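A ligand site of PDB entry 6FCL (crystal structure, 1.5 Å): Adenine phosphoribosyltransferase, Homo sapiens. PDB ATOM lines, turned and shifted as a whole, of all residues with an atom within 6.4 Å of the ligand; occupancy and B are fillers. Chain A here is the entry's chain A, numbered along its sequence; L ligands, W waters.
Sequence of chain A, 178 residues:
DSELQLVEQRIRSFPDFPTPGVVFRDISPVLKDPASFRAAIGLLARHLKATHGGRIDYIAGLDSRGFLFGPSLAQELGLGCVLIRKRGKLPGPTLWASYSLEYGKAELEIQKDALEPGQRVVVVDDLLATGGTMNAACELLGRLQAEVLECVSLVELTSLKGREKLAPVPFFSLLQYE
N of Gly 131 sits at hydrogen-bond distance from O2 of the ligand.
The backbone carbonyl oxygen (O) of Val 23 is in hydrogen-bond range of a nitrogen (N3) of the ligand.
The side-chain hydroxyl of Thr 130 lies within hydrogen-bond range of an oxygen (O1) of the ligand (2.5 Å).
An oxygen (O1) of the ligand lies within hydrogen-bond range of the backbone NH (N) of Thr 130, at 2.9 Å.
OG1 of Thr 133 is in hydrogen-bond range of O3 of the ligand, at 2.7 Å.
N of Arg 25 lies within hydrogen-bond range of N4 of the ligand.
An oxygen (O2) of the ligand lies within hydrogen-bond range of the backbone NH of Ala 129, 2.9 Å away.
An oxygen (O3) of the ligand sits at hydrogen-bond distance from the backbone NH (N) of Gly 132 (3.5 Å).
An oxygen (O7) of the ligand sits at hydrogen-bond distance from the side-chain carboxylate of Asp 126, 2.8 Å away.
NH1 of Arg 65 is in hydrogen-bond range of O7 of the ligand (2.7 Å).
N of Thr 133 is in hydrogen-bond range of O3 of the ligand (2.9 Å).
Residues that only touch the ligand: Phe 24, Leu 157, Leu 127 and Asp 125.
13 residues have an atom within 4 Å of the ligand: Val 23, Phe 24, Arg 25, Arg 65, Asp 125, Asp 126, Leu 127, Ala 129, Thr 130, Gly 131, Gly 132, Thr 133 and Leu 157.
The nearest printed residue that does not touch the ligand is Leu 128 (4.05 Å).
O of Leu 128 sits at hydrogen-bond distance from N of Leu 157 (3.0 Å).
OD2 of Asp 126 is in salt-bridge range of NH1 of Arg 65 (2.6 Å).
The side-chain hydroxyl (OG1) of Thr 130 lies close to the backbone NH (N) of Gly 132 (3.3 Å).
Water W1 lies within hydrogen-bond range of an oxygen (O2) of the ligand (2.7 Å), the backbone NH of Met 134 (2.9 Å) and the backbone NH of Thr 133 (3.4 Å).
Water W3 lies within hydrogen-bond range of O3 of the ligand (2.8 Å), O of Ser 100 (2.8 Å) and OG1 of Thr 130 (3.3 Å).
Water W5 lies within hydrogen-bond range of O6 of the ligand (3.2 Å), N of Arg 65 (3.2 Å) and OG of Ser 64 (3.4 Å).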
ATOM      1  N   PHE A  17     -13.837 -17.483 -23.107  1.00  0.00           N
ATOM      2  CA  PHE A  17     -13.530 -16.385 -24.023  1.00  0.00           C
ATOM      3  C   PHE A  17     -14.784 -15.526 -24.161  1.00  0.00           C
ATOM      4  O   PHE A  17     -15.840 -16.047 -24.484  1.00  0.00           O
ATOM      5  CB  PHE A  17     -13.113 -16.885 -25.404  1.00  0.00           C
ATOM      6  CG  PHE A  17     -12.759 -15.778 -26.356  1.00  0.00           C
ATOM      7  CD1 PHE A  17     -11.469 -15.252 -26.365  1.00  0.00           C
ATOM      8  CD2 PHE A  17     -13.712 -15.220 -27.188  1.00  0.00           C
ATOM      9  CE1 PHE A  17     -11.155 -14.197 -27.211  1.00  0.00           C
ATOM     10  CE2 PHE A  17     -13.398 -14.166 -28.035  1.00  0.00           C
ATOM     11  CZ  PHE A  17     -12.112 -13.664 -28.045  1.00  0.00           C
ATOM     12  N   VAL A  22     -17.541 -17.465 -19.471  1.00  0.00           N
ATOM     13  CA  VAL A  22     -18.284 -17.237 -20.724  1.00  0.00           C
ATOM     14  C   VAL A  22     -17.955 -18.327 -21.734  1.00  0.00           C
ATOM     15  O   VAL A  22     -16.772 -18.678 -21.909  1.00  0.00           O
ATOM     16  CB  VAL A  22     -17.871 -15.895 -21.376  1.00  0.00           C
ATOM     17  CG1 VAL A  22     -18.615 -15.669 -22.675  1.00  0.00           C
ATOM     18  CG2 VAL A  22     -18.093 -14.725 -20.416  1.00  0.00           C
ATOM     19  N   VAL A  23     -18.968 -18.856 -22.408  1.00  0.00           N
ATOM     20  CA  VAL A  23     -18.754 -19.770 -23.529  1.00  0.00           C
ATOM     21  C   VAL A  23     -19.031 -19.041 -24.838  1.00  0.00           C
ATOM     22  O   VAL A  23     -20.165 -18.607 -25.103  1.00  0.00           O
ATOM     23  CB  VAL A  23     -19.620 -21.038 -23.418  1.00  0.00           C
ATOM     24  CG1 VAL A  23     -19.331 -21.958 -24.592  1.00  0.00           C
ATOM     25  CG2 VAL A  23     -19.346 -21.754 -22.105  1.00  0.00           C
ATOM     26  N   PHE A  24     -17.998 -18.894 -25.650  1.00  0.00           N
ATOM     27  CA  PHE A  24     -18.138 -18.204 -26.918  1.00  0.00           C
ATOM     28  C   PHE A  24     -18.648 -19.166 -27.985  1.00  0.00           C
ATOM     29  O   PHE A  24     -18.099 -20.245 -28.188  1.00  0.00           O
ATOM     30  CB  PHE A  24     -16.789 -17.593 -27.365  1.00  0.00           C
ATOM     31  CG  PHE A  24     -16.903 -16.664 -28.533  1.00  0.00           C
ATOM     32  CD1 PHE A  24     -16.862 -17.151 -29.835  1.00  0.00           C
ATOM     33  CD2 PHE A  24     -17.036 -15.297 -28.345  1.00  0.00           C
ATOM     34  CE1 PHE A  24     -16.983 -16.313 -30.914  1.00  0.00           C
ATOM     35  CE2 PHE A  24     -17.147 -14.443 -29.441  1.00  0.00           C
ATOM     36  CZ  PHE A  24     -17.127 -14.952 -30.715  1.00  0.00           C
ATOM     37  N   ARG A  25     -19.708 -18.763 -28.673  1.00  0.00           N
ATOM     38  CA  ARG A  25     -20.266 -19.580 -29.732  1.00  0.00           C
ATOM     39  C   ARG A  25     -19.784 -19.019 -31.061  1.00  0.00           C
ATOM     40  O   ARG A  25     -20.222 -17.962 -31.470  1.00  0.00           O
ATOM     41  CB  ARG A  25     -21.792 -19.568 -29.678  1.00  0.00           C
ATOM     42  CG  ARG A  25     -22.362 -19.855 -28.301  1.00  0.00           C
ATOM     43  CD  ARG A  25     -21.981 -21.231 -27.792  1.00  0.00           C
ATOM     44  NE  ARG A  25     -22.519 -21.442 -26.454  1.00  0.00           N
ATOM     45  CZ  ARG A  25     -22.591 -22.606 -25.834  1.00  0.00           C
ATOM     46  NH1 ARG A  25     -22.195 -23.719 -26.430  1.00  0.00           N
ATOM     47  NH2 ARG A  25     -23.110 -22.665 -24.621  1.00  0.00           N
ATOM     48  N   ASP A  26     -18.923 -19.779 -31.734  1.00  0.00           N
ATOM     49  CA  ASP A  26     -18.263 -19.337 -32.970  1.00  0.00           C
ATOM     50  C   ASP A  26     -18.983 -19.904 -34.203  1.00  0.00           C
ATOM     51  O   ASP A  26     -19.030 -21.120 -34.360  1.00  0.00           O
ATOM     52  CB  ASP A  26     -16.813 -19.817 -32.963  1.00  0.00           C
ATOM     53  CG  ASP A  26     -16.006 -19.353 -34.174  1.00  0.00           C
ATOM     54  OD1 ASP A  26     -16.483 -18.463 -34.909  1.00  0.00           O
ATOM     55  OD2 ASP A  26     -14.913 -19.920 -34.367  1.00  0.00           O
ATOM     56  N   ASP A  63     -24.271  -4.792 -37.747  1.00  0.00           N
ATOM     57  CA  ASP A  63     -22.804  -4.742 -37.689  1.00  0.00           C
ATOM     58  C   ASP A  63     -22.353  -5.519 -36.451  1.00  0.00           C
ATOM     59  O   ASP A  63     -22.880  -5.261 -35.370  1.00  0.00           O
ATOM     60  CB  ASP A  63     -22.417  -3.255 -37.517  1.00  0.00           C
ATOM     61  CG  ASP A  63     -20.974  -2.951 -37.902  1.00  0.00           C
ATOM     62  OD1 ASP A  63     -20.184  -3.877 -38.136  1.00  0.00           O
ATOM     63  OD2 ASP A  63     -20.658  -1.741 -37.978  1.00  0.00           O
ATOM     64  N   SER A  64     -21.385  -6.435 -36.539  1.00  0.00           N
ATOM     65  CA  SER A  64     -20.683  -6.761 -37.774  1.00  0.00           C
ATOM     66  C   SER A  64     -21.011  -8.165 -38.279  1.00  0.00           C
ATOM     67  O   SER A  64     -20.968  -8.442 -39.485  1.00  0.00           O
ATOM     68  CB  SER A  64     -19.169  -6.667 -37.537  1.00  0.00           C
ATOM     69  OG  SER A  64     -18.817  -7.368 -36.367  1.00  0.00           O
ATOM     70  N   ARG A  65     -21.289  -9.085 -37.358  1.00  0.00           N
ATOM     71  CA  ARG A  65     -21.537 -10.472 -37.765  1.00  0.00           C
ATOM     72  C   ARG A  65     -22.914 -10.687 -38.419  1.00  0.00           C
ATOM     73  O   ARG A  65     -23.113 -11.671 -39.132  1.00  0.00           O
ATOM     74  CB  ARG A  65     -21.320 -11.431 -36.595  1.00  0.00           C
ATOM     75  CG  ARG A  65     -19.849 -11.700 -36.278  1.00  0.00           C
ATOM     76  CD  ARG A  65     -19.690 -12.673 -35.121  1.00  0.00           C
ATOM     77  NE  ARG A  65     -19.380 -11.993 -33.868  1.00  0.00           N
ATOM     78  CZ  ARG A  65     -19.735 -12.417 -32.656  1.00  0.00           C
ATOM     79  NH1 ARG A  65     -20.546 -13.459 -32.521  1.00  0.00           N
ATOM     80  NH2 ARG A  65     -19.360 -11.722 -31.586  1.00  0.00           N
ATOM     81  N   TYR A  99     -26.591   1.993 -25.950  1.00  0.00           N
ATOM     82  CA  TYR A  99     -26.991   0.810 -25.196  1.00  0.00           C
ATOM     83  C   TYR A  99     -25.829   0.326 -24.343  1.00  0.00           C
ATOM     84  O   TYR A  99     -24.692   0.788 -24.498  1.00  0.00           O
ATOM     85  CB  TYR A  99     -27.501  -0.301 -26.133  1.00  0.00           C
ATOM     86  CG  TYR A  99     -26.479  -0.824 -27.111  1.00  0.00           C
ATOM     87  CD1 TYR A  99     -26.042  -0.040 -28.180  1.00  0.00           C
ATOM     88  CD2 TYR A  99     -25.950  -2.096 -26.985  1.00  0.00           C
ATOM     89  CE1 TYR A  99     -25.100  -0.511 -29.081  1.00  0.00           C
ATOM     90  CE2 TYR A  99     -25.004  -2.580 -27.890  1.00  0.00           C
ATOM     91  CZ  TYR A  99     -24.585  -1.787 -28.935  1.00  0.00           C
ATOM     92  OH  TYR A  99     -23.648  -2.258 -29.815  1.00  0.00           O
ATOM     93  N   SER A 100     -26.126  -0.575 -23.403  1.00  0.00           N
ATOM     94  CA  SER A 100     -25.111  -1.154 -22.541  1.00  0.00           C
ATOM     95  C   SER A 100     -24.438  -2.327 -23.237  1.00  0.00           C
ATOM     96  O   SER A 100     -25.114  -3.192 -23.814  1.00  0.00           O
ATOM     97  CB  SER A 100     -25.734  -1.648 -21.220  1.00  0.00           C
ATOM     98  OG  SER A 100     -26.232  -0.568 -20.445  1.00  0.00           O
ATOM     99  N   LEU A 101     -23.114  -2.363 -23.195  1.00  0.00           N
ATOM    100  CA  LEU A 101     -22.366  -3.474 -23.770  1.00  0.00           C
ATOM    101  C   LEU A 101     -21.209  -3.791 -22.837  1.00  0.00           C
ATOM    102  O   LEU A 101     -20.358  -2.944 -22.576  1.00  0.00           O
ATOM    103  CB  LEU A 101     -21.852  -3.113 -25.165  1.00  0.00           C
ATOM    104  CG  LEU A 101     -21.038  -4.221 -25.859  1.00  0.00           C
ATOM    105  CD1 LEU A 101     -21.920  -5.418 -26.215  1.00  0.00           C
ATOM    106  CD2 LEU A 101     -20.363  -3.666 -27.099  1.00  0.00           C
ATOM    107  N   ASP A 125     -29.082 -10.903 -36.765  1.00  0.00           N
ATOM    108  CA  ASP A 125     -27.716 -10.924 -36.231  1.00  0.00           C
ATOM    109  C   ASP A 125     -27.347 -12.399 -36.059  1.00  0.00           C
ATOM    110  O   ASP A 125     -28.205 -13.281 -36.190  1.00  0.00           O
ATOM    111  CB  ASP A 125     -27.671 -10.185 -34.884  1.00  0.00           C
ATOM    112  CG  ASP A 125     -26.278  -9.656 -34.525  1.00  0.00           C
ATOM    113  OD1 ASP A 125     -25.294  -9.937 -35.250  1.00  0.00           O
ATOM    114  OD2 ASP A 125     -26.178  -8.977 -33.479  1.00  0.00           O
ATOM    115  N   ASP A 126     -26.081 -12.695 -35.783  1.00  0.00           N
ATOM    116  CA  ASP A 126     -25.683 -14.090 -35.640  1.00  0.00           C
ATOM    117  C   ASP A 126     -26.193 -14.720 -34.346  1.00  0.00           C
ATOM    118  O   ASP A 126     -26.615 -15.870 -34.344  1.00  0.00           O
ATOM    119  CB  ASP A 126     -24.168 -14.278 -35.787  1.00  0.00           C
ATOM    120  CG  ASP A 126     -23.355 -13.682 -34.631  1.00  0.00           C
ATOM    121  OD1 ASP A 126     -23.749 -12.683 -34.015  1.00  0.00           O
ATOM    122  OD2 ASP A 126     -22.244 -14.227 -34.378  1.00  0.00           O
ATOM    123  N   LEU A 127     -26.177 -13.949 -33.255  1.00  0.00           N
ATOM    124  CA  LEU A 127     -26.468 -14.498 -31.951  1.00  0.00           C
ATOM    125  C   LEU A 127     -27.136 -13.469 -31.056  1.00  0.00           C
ATOM    126  O   LEU A 127     -26.712 -12.313 -31.025  1.00  0.00           O
ATOM    127  CB  LEU A 127     -25.149 -14.977 -31.304  1.00  0.00           C
ATOM    128  CG  LEU A 127     -25.200 -15.571 -29.889  1.00  0.00           C
ATOM    129  CD1 LEU A 127     -24.070 -16.583 -29.728  1.00  0.00           C
ATOM    130  CD2 LEU A 127     -25.150 -14.516 -28.785  1.00  0.00           C
ATOM    131  N   LEU A 128     -28.171 -13.923 -30.329  1.00  0.00           N
ATOM    132  CA  LEU A 128     -28.868 -13.119 -29.335  1.00  0.00           C
ATOM    133  C   LEU A 128     -28.432 -13.541 -27.937  1.00  0.00           C
ATOM    134  O   LEU A 128     -28.533 -14.710 -27.579  1.00  0.00           O
ATOM    135  CB  LEU A 128     -30.370 -13.317 -29.449  1.00  0.00           C
ATOM    136  CG  LEU A 128     -31.205 -12.401 -28.530  1.00  0.00           C
ATOM    137  CD1 LEU A 128     -31.331 -11.027 -29.153  1.00  0.00           C
ATOM    138  CD2 LEU A 128     -32.576 -13.024 -28.316  1.00  0.00           C
ATOM    139  N   ALA A 129     -27.935 -12.590 -27.148  1.00  0.00           N
ATOM    140  CA  ALA A 129     -27.484 -12.871 -25.790  1.00  0.00           C
ATOM    141  C   ALA A 129     -28.377 -12.083 -24.840  1.00  0.00           C
ATOM    142  O   ALA A 129     -29.545 -12.452 -24.694  1.00  0.00           O
ATOM    143  CB  ALA A 129     -26.011 -12.504 -25.628  1.00  0.00           C
ATOM    144  N   THR A 130     -27.916 -10.950 -24.300  1.00  0.00           N
ATOM    145  CA  THR A 130     -28.776 -10.143 -23.430  1.00  0.00           C
ATOM    146  C   THR A 130     -29.895  -9.467 -24.211  1.00  0.00           C
ATOM    147  O   THR A 130     -30.921  -9.082 -23.666  1.00  0.00           O
ATOM    148  CB  THR A 130     -28.020  -9.033 -22.667  1.00  0.00           C
ATOM    149  OG1 THR A 130     -27.500  -8.070 -23.589  1.00  0.00           O
ATOM    150  CG2 THR A 130     -26.880  -9.616 -21.844  1.00  0.00           C
ATOM    151  N   GLY A 131     -29.682  -9.292 -25.511  1.00  0.00           N
ATOM    152  CA  GLY A 131     -30.672  -8.632 -26.335  1.00  0.00           C
ATOM    153  C   GLY A 131     -30.497  -7.139 -26.420  1.00  0.00           C
ATOM    154  O   GLY A 131     -31.242  -6.463 -27.127  1.00  0.00           O
ATOM    155  N   GLY A 132     -29.483  -6.619 -25.741  1.00  0.00           N
ATOM    156  CA  GLY A 132     -29.199  -5.185 -25.774  1.00  0.00           C
ATOM    157  C   GLY A 132     -28.967  -4.653 -27.181  1.00  0.00           C
ATOM    158  O   GLY A 132     -29.487  -3.597 -27.547  1.00  0.00           O
ATOM    159  N   THR A 133     -28.173  -5.382 -27.972  1.00  0.00           N
ATOM    160  CA  THR A 133     -27.833  -4.947 -29.332  1.00  0.00           C
ATOM    161  C   THR A 133     -29.060  -4.959 -30.244  1.00  0.00           C
ATOM    162  O   THR A 133     -29.331  -3.991 -30.950  1.00  0.00           O
ATOM    163  CB  THR A 133     -26.724  -5.839 -29.930  1.00  0.00           C
ATOM    164  OG1 THR A 133     -25.566  -5.827 -29.086  1.00  0.00           O
ATOM    165  CG2 THR A 133     -26.327  -5.345 -31.323  1.00  0.00           C
ATOM    166  N   MET A 134     -29.836  -6.037 -30.184  1.00  0.00           N
ATOM    167  CA  MET A 134     -31.034  -6.163 -30.998  1.00  0.00           C
ATOM    168  C   MET A 134     -32.088  -5.139 -30.573  1.00  0.00           C
ATOM    169  O   MET A 134     -32.816  -4.597 -31.406  1.00  0.00           O
ATOM    170  CB  MET A 134     -31.593  -7.578 -30.878  1.00  0.00           C
ATOM    171  CG  MET A 134     -32.009  -8.202 -32.193  1.00  0.00           C
ATOM    172  SD  MET A 134     -31.796 -10.004 -32.145  1.00  0.00           S
ATOM    173  CE  MET A 134     -30.992 -10.305 -33.705  1.00  0.00           C
ATOM    174  N   LEU A 157     -28.893 -17.506 -26.568  1.00  0.00           N
ATOM    175  CA  LEU A 157     -28.470 -17.951 -25.233  1.00  0.00           C
ATOM    176  C   LEU A 157     -29.639 -17.739 -24.245  1.00  0.00           C
ATOM    177  O   LEU A 157     -29.865 -16.634 -23.752  1.00  0.00           O
ATOM    178  CB  LEU A 157     -27.218 -17.210 -24.802  1.00  0.00           C
ATOM    179  CG  LEU A 157     -26.094 -17.232 -25.850  1.00  0.00           C
ATOM    180  CD1 LEU A 157     -24.887 -16.436 -25.368  1.00  0.00           C
ATOM    181  CD2 LEU A 157     -25.693 -18.637 -26.222  1.00  0.00           C
ATOM    182  N   LEU A 160     -30.024 -15.870 -20.726  1.00  0.00           N
ATOM    183  CA  LEU A 160     -29.862 -14.425 -20.641  1.00  0.00           C
ATOM    184  C   LEU A 160     -31.154 -13.634 -20.921  1.00  0.00           C
ATOM    185  O   LEU A 160     -31.155 -12.404 -20.855  1.00  0.00           O
ATOM    186  CB  LEU A 160     -28.741 -13.962 -21.589  1.00  0.00           C
ATOM    187  CG  LEU A 160     -27.379 -14.593 -21.328  1.00  0.00           C
ATOM    188  CD1 LEU A 160     -26.304 -13.992 -22.218  1.00  0.00           C
ATOM    189  CD2 LEU A 160     -26.992 -14.450 -19.860  1.00  0.00           C
HETATM  190  P1  LIG L   1     -26.239  -8.880 -26.710  1.00  0.00           P
HETATM  191  O1  LIG L   1     -25.893  -9.120 -25.244  1.00  0.00           O
HETATM  192  O2  LIG L   1     -27.411  -9.699 -27.180  1.00  0.00           O
HETATM  193  O3  LIG L   1     -26.345  -7.406 -27.039  1.00  0.00           O
HETATM  194  O4  LIG L   1     -24.925  -9.368 -27.459  1.00  0.00           O
HETATM  195  C1  LIG L   1     -25.029  -9.579 -28.848  1.00  0.00           C
HETATM  196  C2  LIG L   1     -23.683  -9.278 -29.471  1.00  0.00           C
HETATM  197  O5  LIG L   1     -22.570  -9.860 -28.771  1.00  0.00           O
HETATM  198  C3  LIG L   1     -23.731  -9.916 -30.821  1.00  0.00           C
HETATM  199  O6  LIG L   1     -22.849  -9.176 -31.656  1.00  0.00           O
HETATM  200  C4  LIG L   1     -23.213 -11.316 -30.545  1.00  0.00           C
HETATM  201  O7  LIG L   1     -22.523 -11.786 -31.702  1.00  0.00           O
HETATM  202  C5  LIG L   1     -22.230 -11.116 -29.385  1.00  0.00           C
HETATM  203  N1  LIG L   1     -22.218 -12.198 -28.351  1.00  0.00           N
HETATM  204  C6  LIG L   1     -22.718 -12.108 -27.099  1.00  0.00           C
HETATM  205  N2  LIG L   1     -22.499 -13.246 -26.398  1.00  0.00           N
HETATM  206  C7  LIG L   1     -21.819 -14.072 -27.236  1.00  0.00           C
HETATM  207  C8  LIG L   1     -21.315 -15.415 -27.108  1.00  0.00           C
HETATM  208  N3  LIG L   1     -21.434 -16.111 -25.955  1.00  0.00           N
HETATM  209  N4  LIG L   1     -20.676 -15.965 -28.231  1.00  0.00           N
HETATM  210  C9  LIG L   1     -20.538 -15.265 -29.380  1.00  0.00           C
HETATM  211  N5  LIG L   1     -21.008 -14.011 -29.513  1.00  0.00           N
HETATM  212  C10 LIG L   1     -21.639 -13.424 -28.474  1.00  0.00           C
HETATM  213  O   HOH W   1     -28.845  -8.522 -29.173  1.00  0.00           O
HETATM  214  O   HOH W   2     -23.441  -9.732 -24.130  1.00  0.00           O
HETATM  215  O   HOH W   3     -25.618  -5.720 -24.979  1.00  0.00           O
HETATM  216  O   HOH W   4     -23.241 -12.919 -23.639  1.00  0.00           O
HETATM  217  O   HOH W   5     -20.891  -8.849 -34.162  1.00  0.00           O
